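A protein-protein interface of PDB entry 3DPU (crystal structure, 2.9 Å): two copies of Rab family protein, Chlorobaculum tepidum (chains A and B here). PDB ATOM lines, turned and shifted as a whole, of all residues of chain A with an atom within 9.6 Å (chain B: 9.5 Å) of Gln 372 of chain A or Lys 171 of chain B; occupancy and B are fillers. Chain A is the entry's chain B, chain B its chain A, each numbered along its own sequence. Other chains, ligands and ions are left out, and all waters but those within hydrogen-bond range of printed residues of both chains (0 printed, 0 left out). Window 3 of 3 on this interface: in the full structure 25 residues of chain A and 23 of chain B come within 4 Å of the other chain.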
ATOM      1  N   ASN A 305     -31.476 -17.384  -7.247  1.00  0.00           N
ATOM      2  CA  ASN A 305     -31.578 -16.765  -5.921  1.00  0.00           C
ATOM      3  C   ASN A 305     -32.945 -16.863  -5.239  1.00  0.00           C
ATOM      4  O   ASN A 305     -33.257 -16.042  -4.378  1.00  0.00           O
ATOM      5  CB  ASN A 305     -31.135 -15.304  -5.984  1.00  0.00           C
ATOM      6  CG  ASN A 305     -29.811 -15.134  -6.675  1.00  0.00           C
ATOM      7  OD1 ASN A 305     -28.766 -15.065  -6.028  1.00  0.00           O
ATOM      8  ND2 ASN A 305     -29.838 -15.078  -7.999  1.00  0.00           N
ATOM      9  N   ASN A 368     -33.516 -22.227  -2.802  1.00  0.00           N
ATOM     10  CA  ASN A 368     -32.668 -21.533  -3.769  1.00  0.00           C
ATOM     11  C   ASN A 368     -32.228 -20.120  -3.350  1.00  0.00           C
ATOM     12  O   ASN A 368     -31.340 -19.542  -3.972  1.00  0.00           O
ATOM     13  CB  ASN A 368     -33.372 -21.483  -5.129  1.00  0.00           C
ATOM     14  CG  ASN A 368     -33.208 -22.759  -5.924  1.00  0.00           C
ATOM     15  OD1 ASN A 368     -33.599 -22.823  -7.093  1.00  0.00           O
ATOM     16  ND2 ASN A 368     -32.624 -23.780  -5.304  1.00  0.00           N
ATOM     17  N   LEU A 369     -32.848 -19.577  -2.301  1.00  0.00           N
ATOM     18  CA  LEU A 369     -32.489 -18.268  -1.750  1.00  0.00           C
ATOM     19  C   LEU A 369     -31.002 -18.157  -1.491  1.00  0.00           C
ATOM     20  O   LEU A 369     -30.369 -19.168  -1.201  1.00  0.00           O
ATOM     21  CB  LEU A 369     -33.220 -18.034  -0.426  1.00  0.00           C
ATOM     22  CG  LEU A 369     -34.710 -17.698  -0.476  1.00  0.00           C
ATOM     23  CD1 LEU A 369     -35.283 -17.746   0.924  1.00  0.00           C
ATOM     24  CD2 LEU A 369     -34.908 -16.334  -1.141  1.00  0.00           C
ATOM     25  N   PRO A 370     -30.440 -16.925  -1.588  1.00  0.00           N
ATOM     26  CA  PRO A 370     -29.030 -16.632  -1.299  1.00  0.00           C
ATOM     27  C   PRO A 370     -28.619 -17.142   0.066  1.00  0.00           C
ATOM     28  O   PRO A 370     -29.463 -17.272   0.950  1.00  0.00           O
ATOM     29  CB  PRO A 370     -29.001 -15.108  -1.281  1.00  0.00           C
ATOM     30  CG  PRO A 370     -30.033 -14.711  -2.223  1.00  0.00           C
ATOM     31  CD  PRO A 370     -31.151 -15.703  -2.010  1.00  0.00           C
ATOM     32  N   THR A 371     -27.340 -17.431   0.248  1.00  0.00           N
ATOM     33  CA  THR A 371     -26.891 -17.871   1.553  1.00  0.00           C
ATOM     34  C   THR A 371     -26.722 -16.683   2.502  1.00  0.00           C
ATOM     35  O   THR A 371     -26.716 -16.850   3.721  1.00  0.00           O
ATOM     36  CB  THR A 371     -25.614 -18.727   1.472  1.00  0.00           C
ATOM     37  OG1 THR A 371     -24.483 -17.899   1.184  1.00  0.00           O
ATOM     38  CG2 THR A 371     -25.759 -19.800   0.411  1.00  0.00           C
ATOM     39  N   GLN A 372     -26.600 -15.487   1.929  1.00  0.00           N
ATOM     40  CA  GLN A 372     -26.512 -14.236   2.690  1.00  0.00           C
ATOM     41  C   GLN A 372     -27.354 -13.165   1.997  1.00  0.00           C
ATOM     42  O   GLN A 372     -27.497 -13.191   0.780  1.00  0.00           O
ATOM     43  CB  GLN A 372     -25.069 -13.748   2.774  1.00  0.00           C
ATOM     44  CG  GLN A 372     -24.041 -14.685   2.171  1.00  0.00           C
ATOM     45  CD  GLN A 372     -22.696 -14.552   2.836  1.00  0.00           C
ATOM     46  OE1 GLN A 372     -22.323 -15.370   3.679  1.00  0.00           O
ATOM     47  NE2 GLN A 372     -21.966 -13.500   2.486  1.00  0.00           N
ATOM     48  N   ILE A 373     -27.899 -12.220   2.762  1.00  0.00           N
ATOM     49  CA  ILE A 373     -28.649 -11.105   2.164  1.00  0.00           C
ATOM     50  C   ILE A 373     -28.177  -9.729   2.651  1.00  0.00           C
ATOM     51  O   ILE A 373     -27.522  -9.617   3.685  1.00  0.00           O
ATOM     52  CB  ILE A 373     -30.171 -11.254   2.358  1.00  0.00           C
ATOM     53  CG1 ILE A 373     -30.504 -11.390   3.848  1.00  0.00           C
ATOM     54  CG2 ILE A 373     -30.705 -12.421   1.510  1.00  0.00           C
ATOM     55  CD1 ILE A 373     -31.971 -11.308   4.147  1.00  0.00           C
ATOM     56  N   ASP A 374     -28.515  -8.688   1.896  1.00  0.00           N
ATOM     57  CA  ASP A 374     -28.033  -7.342   2.184  1.00  0.00           C
ATOM     58  C   ASP A 374     -28.786  -6.612   3.299  1.00  0.00           C
ATOM     59  O   ASP A 374     -28.271  -5.637   3.853  1.00  0.00           O
ATOM     60  CB  ASP A 374     -28.024  -6.502   0.907  1.00  0.00           C
ATOM     61  CG  ASP A 374     -26.957  -6.962  -0.091  1.00  0.00           C
ATOM     62  OD1 ASP A 374     -26.031  -7.720   0.292  1.00  0.00           O
ATOM     63  OD2 ASP A 374     -27.039  -6.560  -1.270  1.00  0.00           O
ATOM     64  N   ASN A 375     -29.986  -7.085   3.643  1.00  0.00           N
ATOM     65  CA  ASN A 375     -30.799  -6.435   4.665  1.00  0.00           C
ATOM     66  C   ASN A 375     -31.106  -7.276   5.905  1.00  0.00           C
ATOM     67  O   ASN A 375     -32.171  -7.136   6.495  1.00  0.00           O
ATOM     68  CB  ASN A 375     -32.087  -5.884   4.055  1.00  0.00           C
ATOM     69  CG  ASN A 375     -32.968  -6.959   3.474  1.00  0.00           C
ATOM     70  OD1 ASN A 375     -32.532  -8.073   3.239  1.00  0.00           O
ATOM     71  ND2 ASN A 375     -34.221  -6.622   3.228  1.00  0.00           N
ATOM     72  N   GLU A 376     -30.175  -8.130   6.314  1.00  0.00           N
ATOM     73  CA  GLU A 376     -30.314  -8.845   7.587  1.00  0.00           C
ATOM     74  C   GLU A 376     -30.172  -7.900   8.781  1.00  0.00           C
ATOM     75  O   GLU A 376     -29.178  -7.189   8.876  1.00  0.00           O
ATOM     76  CB  GLU A 376     -29.271  -9.957   7.709  1.00  0.00           C
ATOM     77  CG  GLU A 376     -29.486 -10.836   8.930  1.00  0.00           C
ATOM     78  CD  GLU A 376     -28.552 -12.018   8.994  1.00  0.00           C
ATOM     79  OE1 GLU A 376     -28.418 -12.580  10.106  1.00  0.00           O
ATOM     80  OE2 GLU A 376     -27.951 -12.386   7.953  1.00  0.00           O
ATOM     81  N   ARG A 413     -38.415  -9.062   2.402  1.00  0.00           N
ATOM     82  CA  ARG A 413     -37.529 -10.012   1.730  1.00  0.00           C
ATOM     83  C   ARG A 413     -36.408 -10.490   2.670  1.00  0.00           C
ATOM     84  O   ARG A 413     -35.380 -10.984   2.209  1.00  0.00           O
ATOM     85  CB  ARG A 413     -36.946  -9.368   0.468  1.00  0.00           C
ATOM     86  CG  ARG A 413     -37.966  -9.027  -0.619  1.00  0.00           C
ATOM     87  CD  ARG A 413     -37.901 -10.062  -1.722  1.00  0.00           C
ATOM     88  NE  ARG A 413     -38.874  -9.858  -2.797  1.00  0.00           N
ATOM     89  CZ  ARG A 413     -38.711  -9.030  -3.826  1.00  0.00           C
ATOM     90  NH1 ARG A 413     -37.622  -8.280  -3.926  1.00  0.00           N
ATOM     91  NH2 ARG A 413     -39.655  -8.942  -4.748  1.00  0.00           N
ATOM     92  N   MET A 414     -36.611 -10.337   3.986  1.00  0.00           N
ATOM     93  CA  MET A 414     -35.611 -10.733   4.990  1.00  0.00           C
ATOM     94  C   MET A 414     -35.674 -12.235   5.169  1.00  0.00           C
ATOM     95  O   MET A 414     -36.216 -12.752   6.150  1.00  0.00           O
ATOM     96  CB  MET A 414     -35.805  -9.998   6.319  1.00  0.00           C
ATOM     97  CG  MET A 414     -35.706  -8.490   6.178  1.00  0.00           C
ATOM     98  SD  MET A 414     -35.726  -7.535   7.709  1.00  0.00           S
ATOM     99  CE  MET A 414     -35.432  -5.878   7.078  1.00  0.00           C
ATOM    100  N   GLN A 415     -35.124 -12.925   4.176  1.00  0.00           N
ATOM    101  CA  GLN A 415     -35.119 -14.380   4.119  1.00  0.00           C
ATOM    102  C   GLN A 415     -33.905 -14.824   3.321  1.00  0.00           C
ATOM    103  O   GLN A 415     -33.703 -14.372   2.200  1.00  0.00           O
ATOM    104  CB  GLN A 415     -36.416 -14.914   3.483  1.00  0.00           C
ATOM    105  CG  GLN A 415     -36.672 -14.402   2.085  1.00  0.00           C
ATOM    106  CD  GLN A 415     -38.058 -14.693   1.548  1.00  0.00           C
ATOM    107  OE1 GLN A 415     -38.651 -15.737   1.808  1.00  0.00           O
ATOM    108  NE2 GLN A 415     -38.569 -13.763   0.754  1.00  0.00           N
ATOM    109  N   TRP A 416     -33.085 -15.681   3.913  1.00  0.00           N
ATOM    110  CA  TRP A 416     -31.963 -16.267   3.189  1.00  0.00           C
ATOM    111  C   TRP A 416     -32.064 -17.789   3.280  1.00  0.00           C
ATOM    112  O   TRP A 416     -33.056 -18.296   3.785  1.00  0.00           O
ATOM    113  CB  TRP A 416     -30.625 -15.715   3.697  1.00  0.00           C
ATOM    114  CG  TRP A 416     -30.378 -15.941   5.131  1.00  0.00           C
ATOM    115  CD1 TRP A 416     -29.546 -16.867   5.675  1.00  0.00           C
ATOM    116  CD2 TRP A 416     -30.967 -15.230   6.225  1.00  0.00           C
ATOM    117  NE1 TRP A 416     -29.576 -16.784   7.047  1.00  0.00           N
ATOM    118  CE2 TRP A 416     -30.436 -15.784   7.413  1.00  0.00           C
ATOM    119  CE3 TRP A 416     -31.900 -14.181   6.320  1.00  0.00           C
ATOM    120  CZ2 TRP A 416     -30.802 -15.333   8.682  1.00  0.00           C
ATOM    121  CZ3 TRP A 416     -32.262 -13.721   7.588  1.00  0.00           C
ATOM    122  CH2 TRP A 416     -31.706 -14.302   8.753  1.00  0.00           C
ATOM    123  N   ARG A 417     -31.069 -18.516   2.788  1.00  0.00           N
ATOM    124  CA  ARG A 417     -31.160 -19.971   2.773  1.00  0.00           C
ATOM    125  C   ARG A 417     -31.294 -20.591   4.159  1.00  0.00           C
ATOM    126  O   ARG A 417     -31.973 -21.610   4.347  1.00  0.00           O
ATOM    127  CB  ARG A 417     -29.969 -20.592   2.064  1.00  0.00           C
ATOM    128  CG  ARG A 417     -30.386 -21.715   1.155  1.00  0.00           C
ATOM    129  CD  ARG A 417     -29.193 -22.404   0.592  1.00  0.00           C
ATOM    130  NE  ARG A 417     -29.363 -22.655  -0.829  1.00  0.00           N
ATOM    131  CZ  ARG A 417     -28.971 -21.826  -1.784  1.00  0.00           C
ATOM    132  NH1 ARG A 417     -28.386 -20.682  -1.481  1.00  0.00           N
ATOM    133  NH2 ARG A 417     -29.176 -22.137  -3.050  1.00  0.00           N
ATOM    134  N   TYR A 418     -30.656 -19.963   5.134  1.00  0.00           N
ATOM    135  CA  TYR A 418     -30.559 -20.555   6.447  1.00  0.00           C
ATOM    136  C   TYR A 418     -31.266 -19.718   7.488  1.00  0.00           C
ATOM    137  O   TYR A 418     -31.023 -19.858   8.684  1.00  0.00           O
ATOM    138  CB  TYR A 418     -29.094 -20.768   6.807  1.00  0.00           C
ATOM    139  CG  TYR A 418     -28.329 -21.602   5.799  1.00  0.00           C
ATOM    140  CD1 TYR A 418     -28.620 -22.969   5.609  1.00  0.00           C
ATOM    141  CD2 TYR A 418     -27.297 -21.034   5.049  1.00  0.00           C
ATOM    142  CE1 TYR A 418     -27.903 -23.745   4.679  1.00  0.00           C
ATOM    143  CE2 TYR A 418     -26.565 -21.802   4.130  1.00  0.00           C
ATOM    144  CZ  TYR A 418     -26.875 -23.151   3.948  1.00  0.00           C
ATOM    145  OH  TYR A 418     -26.143 -23.878   3.034  1.00  0.00           O
ATOM    146  N   GLY A 419     -32.168 -18.859   7.052  1.00  0.00           N
ATOM    147  CA  GLY A 419     -32.932 -18.116   8.029  1.00  0.00           C
ATOM    148  C   GLY A 419     -34.009 -17.237   7.464  1.00  0.00           C
ATOM    149  O   GLY A 419     -34.169 -17.138   6.242  1.00  0.00           O
ATOM    150  N   SER B 165     -27.959 -22.361  -8.386  1.00  0.00           N
ATOM    151  CA  SER B 165     -28.276 -21.828  -7.065  1.00  0.00           C
ATOM    152  C   SER B 165     -27.235 -22.158  -5.995  1.00  0.00           C
ATOM    153  O   SER B 165     -27.318 -21.640  -4.882  1.00  0.00           O
ATOM    154  CB  SER B 165     -29.645 -22.330  -6.604  1.00  0.00           C
ATOM    155  OG  SER B 165     -29.549 -23.672  -6.185  1.00  0.00           O
ATOM    156  N   ASN B 167     -24.483 -22.223  -3.417  1.00  0.00           N
ATOM    157  CA  ASN B 167     -23.562 -21.348  -2.709  1.00  0.00           C
ATOM    158  C   ASN B 167     -23.401 -21.797  -1.267  1.00  0.00           C
ATOM    159  O   ASN B 167     -24.001 -22.781  -0.857  1.00  0.00           O
ATOM    160  CB  ASN B 167     -24.033 -19.894  -2.782  1.00  0.00           C
ATOM    161  CG  ASN B 167     -22.901 -18.926  -3.103  1.00  0.00           C
ATOM    162  OD1 ASN B 167     -23.019 -18.121  -4.030  1.00  0.00           O
ATOM    163  ND2 ASN B 167     -21.794 -19.010  -2.357  1.00  0.00           N
ATOM    164  N   ILE B 168     -22.586 -21.083  -0.503  1.00  0.00           N
ATOM    165  CA  ILE B 168     -22.313 -21.439   0.880  1.00  0.00           C
ATOM    166  C   ILE B 168     -22.318 -20.192   1.770  1.00  0.00           C
ATOM    167  O   ILE B 168     -22.075 -19.080   1.293  1.00  0.00           O
ATOM    168  CB  ILE B 168     -20.962 -22.161   1.008  1.00  0.00           C
ATOM    169  CG1 ILE B 168     -19.836 -21.305   0.407  1.00  0.00           C
ATOM    170  CG2 ILE B 168     -21.027 -23.544   0.368  1.00  0.00           C
ATOM    171  CD1 ILE B 168     -18.443 -21.765   0.755  1.00  0.00           C
ATOM    172  N   GLU B 169     -22.594 -20.371   3.066  1.00  0.00           N
ATOM    173  CA  GLU B 169     -22.590 -19.239   4.013  1.00  0.00           C
ATOM    174  C   GLU B 169     -21.179 -18.634   4.145  1.00  0.00           C
ATOM    175  O   GLU B 169     -20.490 -18.824   5.154  1.00  0.00           O
ATOM    176  CB  GLU B 169     -23.200 -19.626   5.372  1.00  0.00           C
ATOM    177  N   GLN B 170     -20.787 -17.910   3.086  1.00  0.00           N
ATOM    178  CA  GLN B 170     -19.500 -17.221   2.960  1.00  0.00           C
ATOM    179  C   GLN B 170     -19.126 -16.314   4.127  1.00  0.00           C
ATOM    180  O   GLN B 170     -18.147 -16.603   4.804  1.00  0.00           O
ATOM    181  CB  GLN B 170     -19.436 -16.441   1.650  1.00  0.00           C
ATOM    182  CG  GLN B 170     -19.268 -17.325   0.435  1.00  0.00           C
ATOM    183  CD  GLN B 170     -19.199 -16.551  -0.863  1.00  0.00           C
ATOM    184  OE1 GLN B 170     -18.813 -15.385  -0.886  1.00  0.00           O
ATOM    185  NE2 GLN B 170     -19.566 -17.206  -1.959  1.00  0.00           N
ATOM    186  N   LYS B 171     -19.886 -15.240   4.365  1.00  0.00           N
ATOM    187  CA  LYS B 171     -19.616 -14.341   5.497  1.00  0.00           C
ATOM    188  C   LYS B 171     -19.302 -15.139   6.757  1.00  0.00           C
ATOM    189  O   LYS B 171     -18.227 -14.990   7.320  1.00  0.00           O
ATOM    190  CB  LYS B 171     -20.763 -13.350   5.749  1.00  0.00           C
ATOM    191  N   LYS B 172     -20.216 -16.016   7.163  1.00  0.00           N
ATOM    192  CA  LYS B 172     -20.027 -16.824   8.368  1.00  0.00           C
ATOM    193  C   LYS B 172     -18.741 -17.649   8.269  1.00  0.00           C
ATOM    194  O   LYS B 172     -17.942 -17.672   9.213  1.00  0.00           O
ATOM    195  CB  LYS B 172     -21.250 -17.715   8.660  1.00  0.00           C
ATOM    196  N   ILE B 173     -18.527 -18.294   7.123  1.00  0.00           N
ATOM    197  CA  ILE B 173     -17.348 -19.138   6.932  1.00  0.00           C
ATOM    198  C   ILE B 173     -16.044 -18.340   6.987  1.00  0.00           C
ATOM    199  O   ILE B 173     -15.061 -18.820   7.532  1.00  0.00           O
ATOM    200  CB  ILE B 173     -17.431 -19.967   5.641  1.00  0.00           C
ATOM    201  CG1 ILE B 173     -18.370 -21.153   5.850  1.00  0.00           C
ATOM    202  CG2 ILE B 173     -16.072 -20.489   5.253  1.00  0.00           C
ATOM    203  CD1 ILE B 173     -18.706 -21.923   4.569  1.00  0.00           C
ATOM    204  N   ASN B 174     -16.049 -17.128   6.438  1.00  0.00           N
ATOM    205  CA  ASN B 174     -14.859 -16.276   6.416  1.00  0.00           C
ATOM    206  C   ASN B 174     -14.551 -15.682   7.800  1.00  0.00           C
ATOM    207  O   ASN B 174     -13.388 -15.498   8.158  1.00  0.00           O
ATOM    208  CB  ASN B 174     -14.995 -15.169   5.356  1.00  0.00           C
ATOM    209  CG  ASN B 174     -13.723 -14.324   5.211  1.00  0.00           C
ATOM    210  OD1 ASN B 174     -12.825 -14.667   4.452  1.00  0.00           O
ATOM    211  ND2 ASN B 174     -13.653 -13.219   5.938  1.00  0.00           N
ATOM    212  N   GLU B 175     -15.594 -15.390   8.570  1.00  0.00           N
ATOM    213  CA  GLU B 175     -15.431 -14.930   9.947  1.00  0.00           C
ATOM    214  C   GLU B 175     -14.735 -16.018  10.790  1.00  0.00           C
ATOM    215  O   GLU B 175     -13.764 -15.743  11.505  1.00  0.00           O
ATOM    216  CB  GLU B 175     -16.789 -14.529  10.538  1.00  0.00           C
ATOM    217  CG  GLU B 175     -16.755 -14.108  12.003  1.00  0.00           C
ATOM    218  CD  GLU B 175     -18.154 -13.863  12.599  1.00  0.00           C
ATOM    219  OE1 GLU B 175     -18.263 -13.693  13.847  1.00  0.00           O
ATOM    220  OE2 GLU B 175     -19.151 -13.840  11.820  1.00  0.00           O
ATOM    221  N   ARG B 176     -15.221 -17.255  10.670  1.00  0.00           N
ATOM    222  CA  ARG B 176     -14.678 -18.394  11.403  1.00  0.00           C
ATOM    223  C   ARG B 176     -13.282 -18.780  10.913  1.00  0.00           C
ATOM    224  O   ARG B 176     -12.463 -19.256  11.687  1.00  0.00           O
ATOM    225  CB  ARG B 176     -15.640 -19.590  11.299  1.00  0.00           C
ATOM    226  CG  ARG B 176     -15.155 -20.913  11.919  1.00  0.00           C
ATOM    227  CD  ARG B 176     -14.757 -20.821  13.416  1.00  0.00           C
ATOM    228  NE  ARG B 176     -14.294 -22.117  13.912  1.00  0.00           N
ATOM    229  CZ  ARG B 176     -13.033 -22.552  13.863  1.00  0.00           C
ATOM    230  NH1 ARG B 176     -12.067 -21.795  13.365  1.00  0.00           N
ATOM    231  NH2 ARG B 176     -12.729 -23.760  14.318  1.00  0.00           N
ATOM    232  N   PHE B 177     -13.021 -18.570   9.626  1.00  0.00           N
ATOM    233  CA  PHE B 177     -11.764 -18.978   9.015  1.00  0.00           C
ATOM    234  C   PHE B 177     -11.115 -17.787   8.308  1.00  0.00           C
ATOM    235  O   PHE B 177     -11.064 -17.738   7.074  1.00  0.00           O
ATOM    236  CB  PHE B 177     -11.992 -20.147   8.039  1.00  0.00           C
ATOM    237  CG  PHE B 177     -12.578 -21.374   8.690  1.00  0.00           C
ATOM    238  CD1 PHE B 177     -13.889 -21.763   8.422  1.00  0.00           C
ATOM    239  CD2 PHE B 177     -11.823 -22.134   9.591  1.00  0.00           C
ATOM    240  CE1 PHE B 177     -14.443 -22.890   9.027  1.00  0.00           C
ATOM    241  CE2 PHE B 177     -12.372 -23.266  10.202  1.00  0.00           C
ATOM    242  CZ  PHE B 177     -13.697 -23.637   9.922  1.00  0.00           C
ATOM    243  N   PRO B 178     -10.604 -16.817   9.087  1.00  0.00           N
ATOM    244  CA  PRO B 178     -10.034 -15.623   8.467  1.00  0.00           C
ATOM    245  C   PRO B 178      -8.919 -15.866   7.433  1.00  0.00           C
ATOM    246  O   PRO B 178      -8.565 -14.942   6.712  1.00  0.00           O
ATOM    247  CB  PRO B 178      -9.507 -14.817   9.668  1.00  0.00           C
ATOM    248  CG  PRO B 178      -9.434 -15.790  10.805  1.00  0.00           C
ATOM    249  CD  PRO B 178     -10.528 -16.759  10.560  1.00  0.00           C
ATOM    250  N   ILE B 180      -9.205 -17.500   4.760  1.00  0.00           N
ATOM    251  CA  ILE B 180      -9.822 -17.566   3.444  1.00  0.00           C
ATOM    252  C   ILE B 180      -9.770 -16.186   2.794  1.00  0.00           C
ATOM    253  O   ILE B 180      -9.713 -16.077   1.573  1.00  0.00           O
ATOM    254  CB  ILE B 180     -11.270 -18.049   3.538  1.00  0.00           C
ATOM    255  CG1 ILE B 180     -11.297 -19.495   4.040  1.00  0.00           C
ATOM    256  CG2 ILE B 180     -11.989 -17.908   2.193  1.00  0.00           C
ATOM    257  CD1 ILE B 180     -12.694 -20.091   4.133  1.00  0.00           C
ATOM    258  N   GLU B 181      -9.783 -15.141   3.623  1.00  0.00           N
ATOM    259  CA  GLU B 181      -9.757 -13.748   3.171  1.00  0.00           C
ATOM    260  C   GLU B 181     -10.656 -13.504   1.965  1.00  0.00           C
ATOM    261  O   GLU B 181     -10.259 -12.836   1.009  1.00  0.00           O
ATOM    262  CB  GLU B 181      -8.332 -13.303   2.863  1.00  0.00           C
ATOM    263  CG  GLU B 181      -7.374 -13.350   4.046  1.00  0.00           C
ATOM    264  CD  GLU B 181      -6.065 -12.638   3.737  1.00  0.00           C
ATOM    265  OE1 GLU B 181      -5.063 -13.328   3.410  1.00  0.00           O
ATOM    266  OE2 GLU B 181      -6.051 -11.385   3.797  1.00  0.00           O
ATOM    267  N   ASN B 182     -11.863 -14.064   2.021  1.00  0.00           N
ATOM    268  CA  ASN B 182     -12.880 -13.915   0.975  1.00  0.00           C
ATOM    269  C   ASN B 182     -12.498 -14.449  -0.406  1.00  0.00           C
ATOM    270  O   ASN B 182     -13.035 -14.008  -1.420  1.00  0.00           O
ATOM    271  CB  ASN B 182     -13.355 -12.464   0.883  1.00  0.00           C
ATOM    272  CG  ASN B 182     -13.993 -11.993   2.157  1.00  0.00           C
ATOM    273  OD1 ASN B 182     -14.927 -12.619   2.662  1.00  0.00           O
ATOM    274  ND2 ASN B 182     -13.486 -10.886   2.702  1.00  0.00           N
ATOM    275  N   PHE B 184     -13.458 -16.832  -2.309  1.00  0.00           N
ATOM    276  CA  PHE B 184     -14.493 -17.794  -2.747  1.00  0.00           C
ATOM    277  C   PHE B 184     -14.739 -17.668  -4.244  1.00  0.00           C
ATOM    278  O   PHE B 184     -14.798 -16.564  -4.780  1.00  0.00           O
ATOM    279  CB  PHE B 184     -15.835 -17.570  -2.039  1.00  0.00           C
ATOM    280  CG  PHE B 184     -15.775 -17.653  -0.540  1.00  0.00           C
ATOM    281  CD1 PHE B 184     -15.622 -16.502   0.224  1.00  0.00           C
ATOM    282  CD2 PHE B 184     -15.906 -18.876   0.109  1.00  0.00           C
ATOM    283  CE1 PHE B 184     -15.575 -16.572   1.606  1.00  0.00           C
ATOM    284  CE2 PHE B 184     -15.856 -18.954   1.495  1.00  0.00           C
ATOM    285  CZ  PHE B 184     -15.695 -17.801   2.244  1.00  0.00           C
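The side-chain hydroxyl (OG) of Ser 165 of chain B lies within hydrogen-bond range of the side-chain amide nitrogen (ND2) of Asn 368 of chain A (3.2 Å).
The guanidinium group (NH2) of Arg 417 of chain A is in hydrogen-bond range of the backbone carbonyl oxygen (O) of Ser 165 of chain B, 2.7 Å away.
The backbone carbonyl oxygen (O) of Ile 168 of chain B lies within hydrogen-bond range of the side-chain hydroxyl (OG1) of Thr 371 of chain A, at 2.7 Å.
N of Gln 170 of chain B is in hydrogen-bond range of OE1 of Gln 372 of chain A (3.0 Å).
The backbone NH of Lys 171 of chain B sits at hydrogen-bond distance from the side-chain amide oxygen of Gln 372 of chain A, at 2.5 Å.
NE2 of Gln 170 of chain B sits close to ND2 of Asn 167 of chain B (2.9 Å).
O of Leu 369 of chain A lies within hydrogen-bond range of NH1 of Arg 417 of chain A (2.5 Å).
The backbone carbonyl oxygen of Pro 370 of chain A lies within hydrogen-bond range of the backbone NH of Arg 417 of chain A.
Asn 167 of chain B touches Thr 371 of chain A.
Thr 371 of chain A touches Glu 169 of chain B (OG1 to N, 3.6 Å).
Gln 372 of chain A touches Glu 169 of chain B.
Of the printed residues of chain B, Gln 372 of chain A touches Glu 169, Gln 170 and Lys 171.
Lys 171 of chain B touches one residue of chain A.
No residue of chain B comes within 4 Å of Pro 370 of chain A.
Of chain B, only Asn 167 (3.5 Å), Ile 168 (2.7 Å) and Glu 169 (3.6 Å) come within 4 Å of Thr 371 of chain A.
No residue of chain B comes within 4 Å of Ile 373 of chain A.
Of chain A, only Thr 371 and Gln 372 come within 4 Å of Glu 169 of chain B.
No residue of chain A comes within 4 Å of Lys 172 of chain B.
Of the printed residues of chain A, Ile 168 of chain B touches Thr 371.
Of the printed residues of chain A, Ser 165 of chain B touches Asn 368 (3.2 Å) and Arg 417 (2.7 Å).
Of the printed residues of chain B, Arg 417 of chain A touches Ser 165.
Printed residues of chain B within 4 Å of Asn 368 of chain A: Ser 165.
Of the printed residues of chain A, Asn 167 of chain B touches Thr 371.
Ile 180 of chain B touches none of the printed residues of chain A.
The nearest residue of chain B that does not touch Gln 372 of chain A is Lys 172 of chain B (4.1 Å).
The nearest residue of chain A that does not touch Lys 171 of chain B is Thr 371 of chain A (6.2 Å).
The nearest printed residue of chain A that does not touch Ser 165 of chain B is Asn 305 of chain A (5.3 Å).
Printed residues of chain A that touch a printed residue of chain B: Asn 368, Thr 371, Gln 372 and Arg 417.
Along chain A the printed residues that touch a printed residue of chain B span positions 368 to 417.
Among the printed residues, no Asp or Glu carboxylate lies within 4 Å of a Lys or Arg side-chain nitrogen of the other chain.
No position is printed for both chains.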
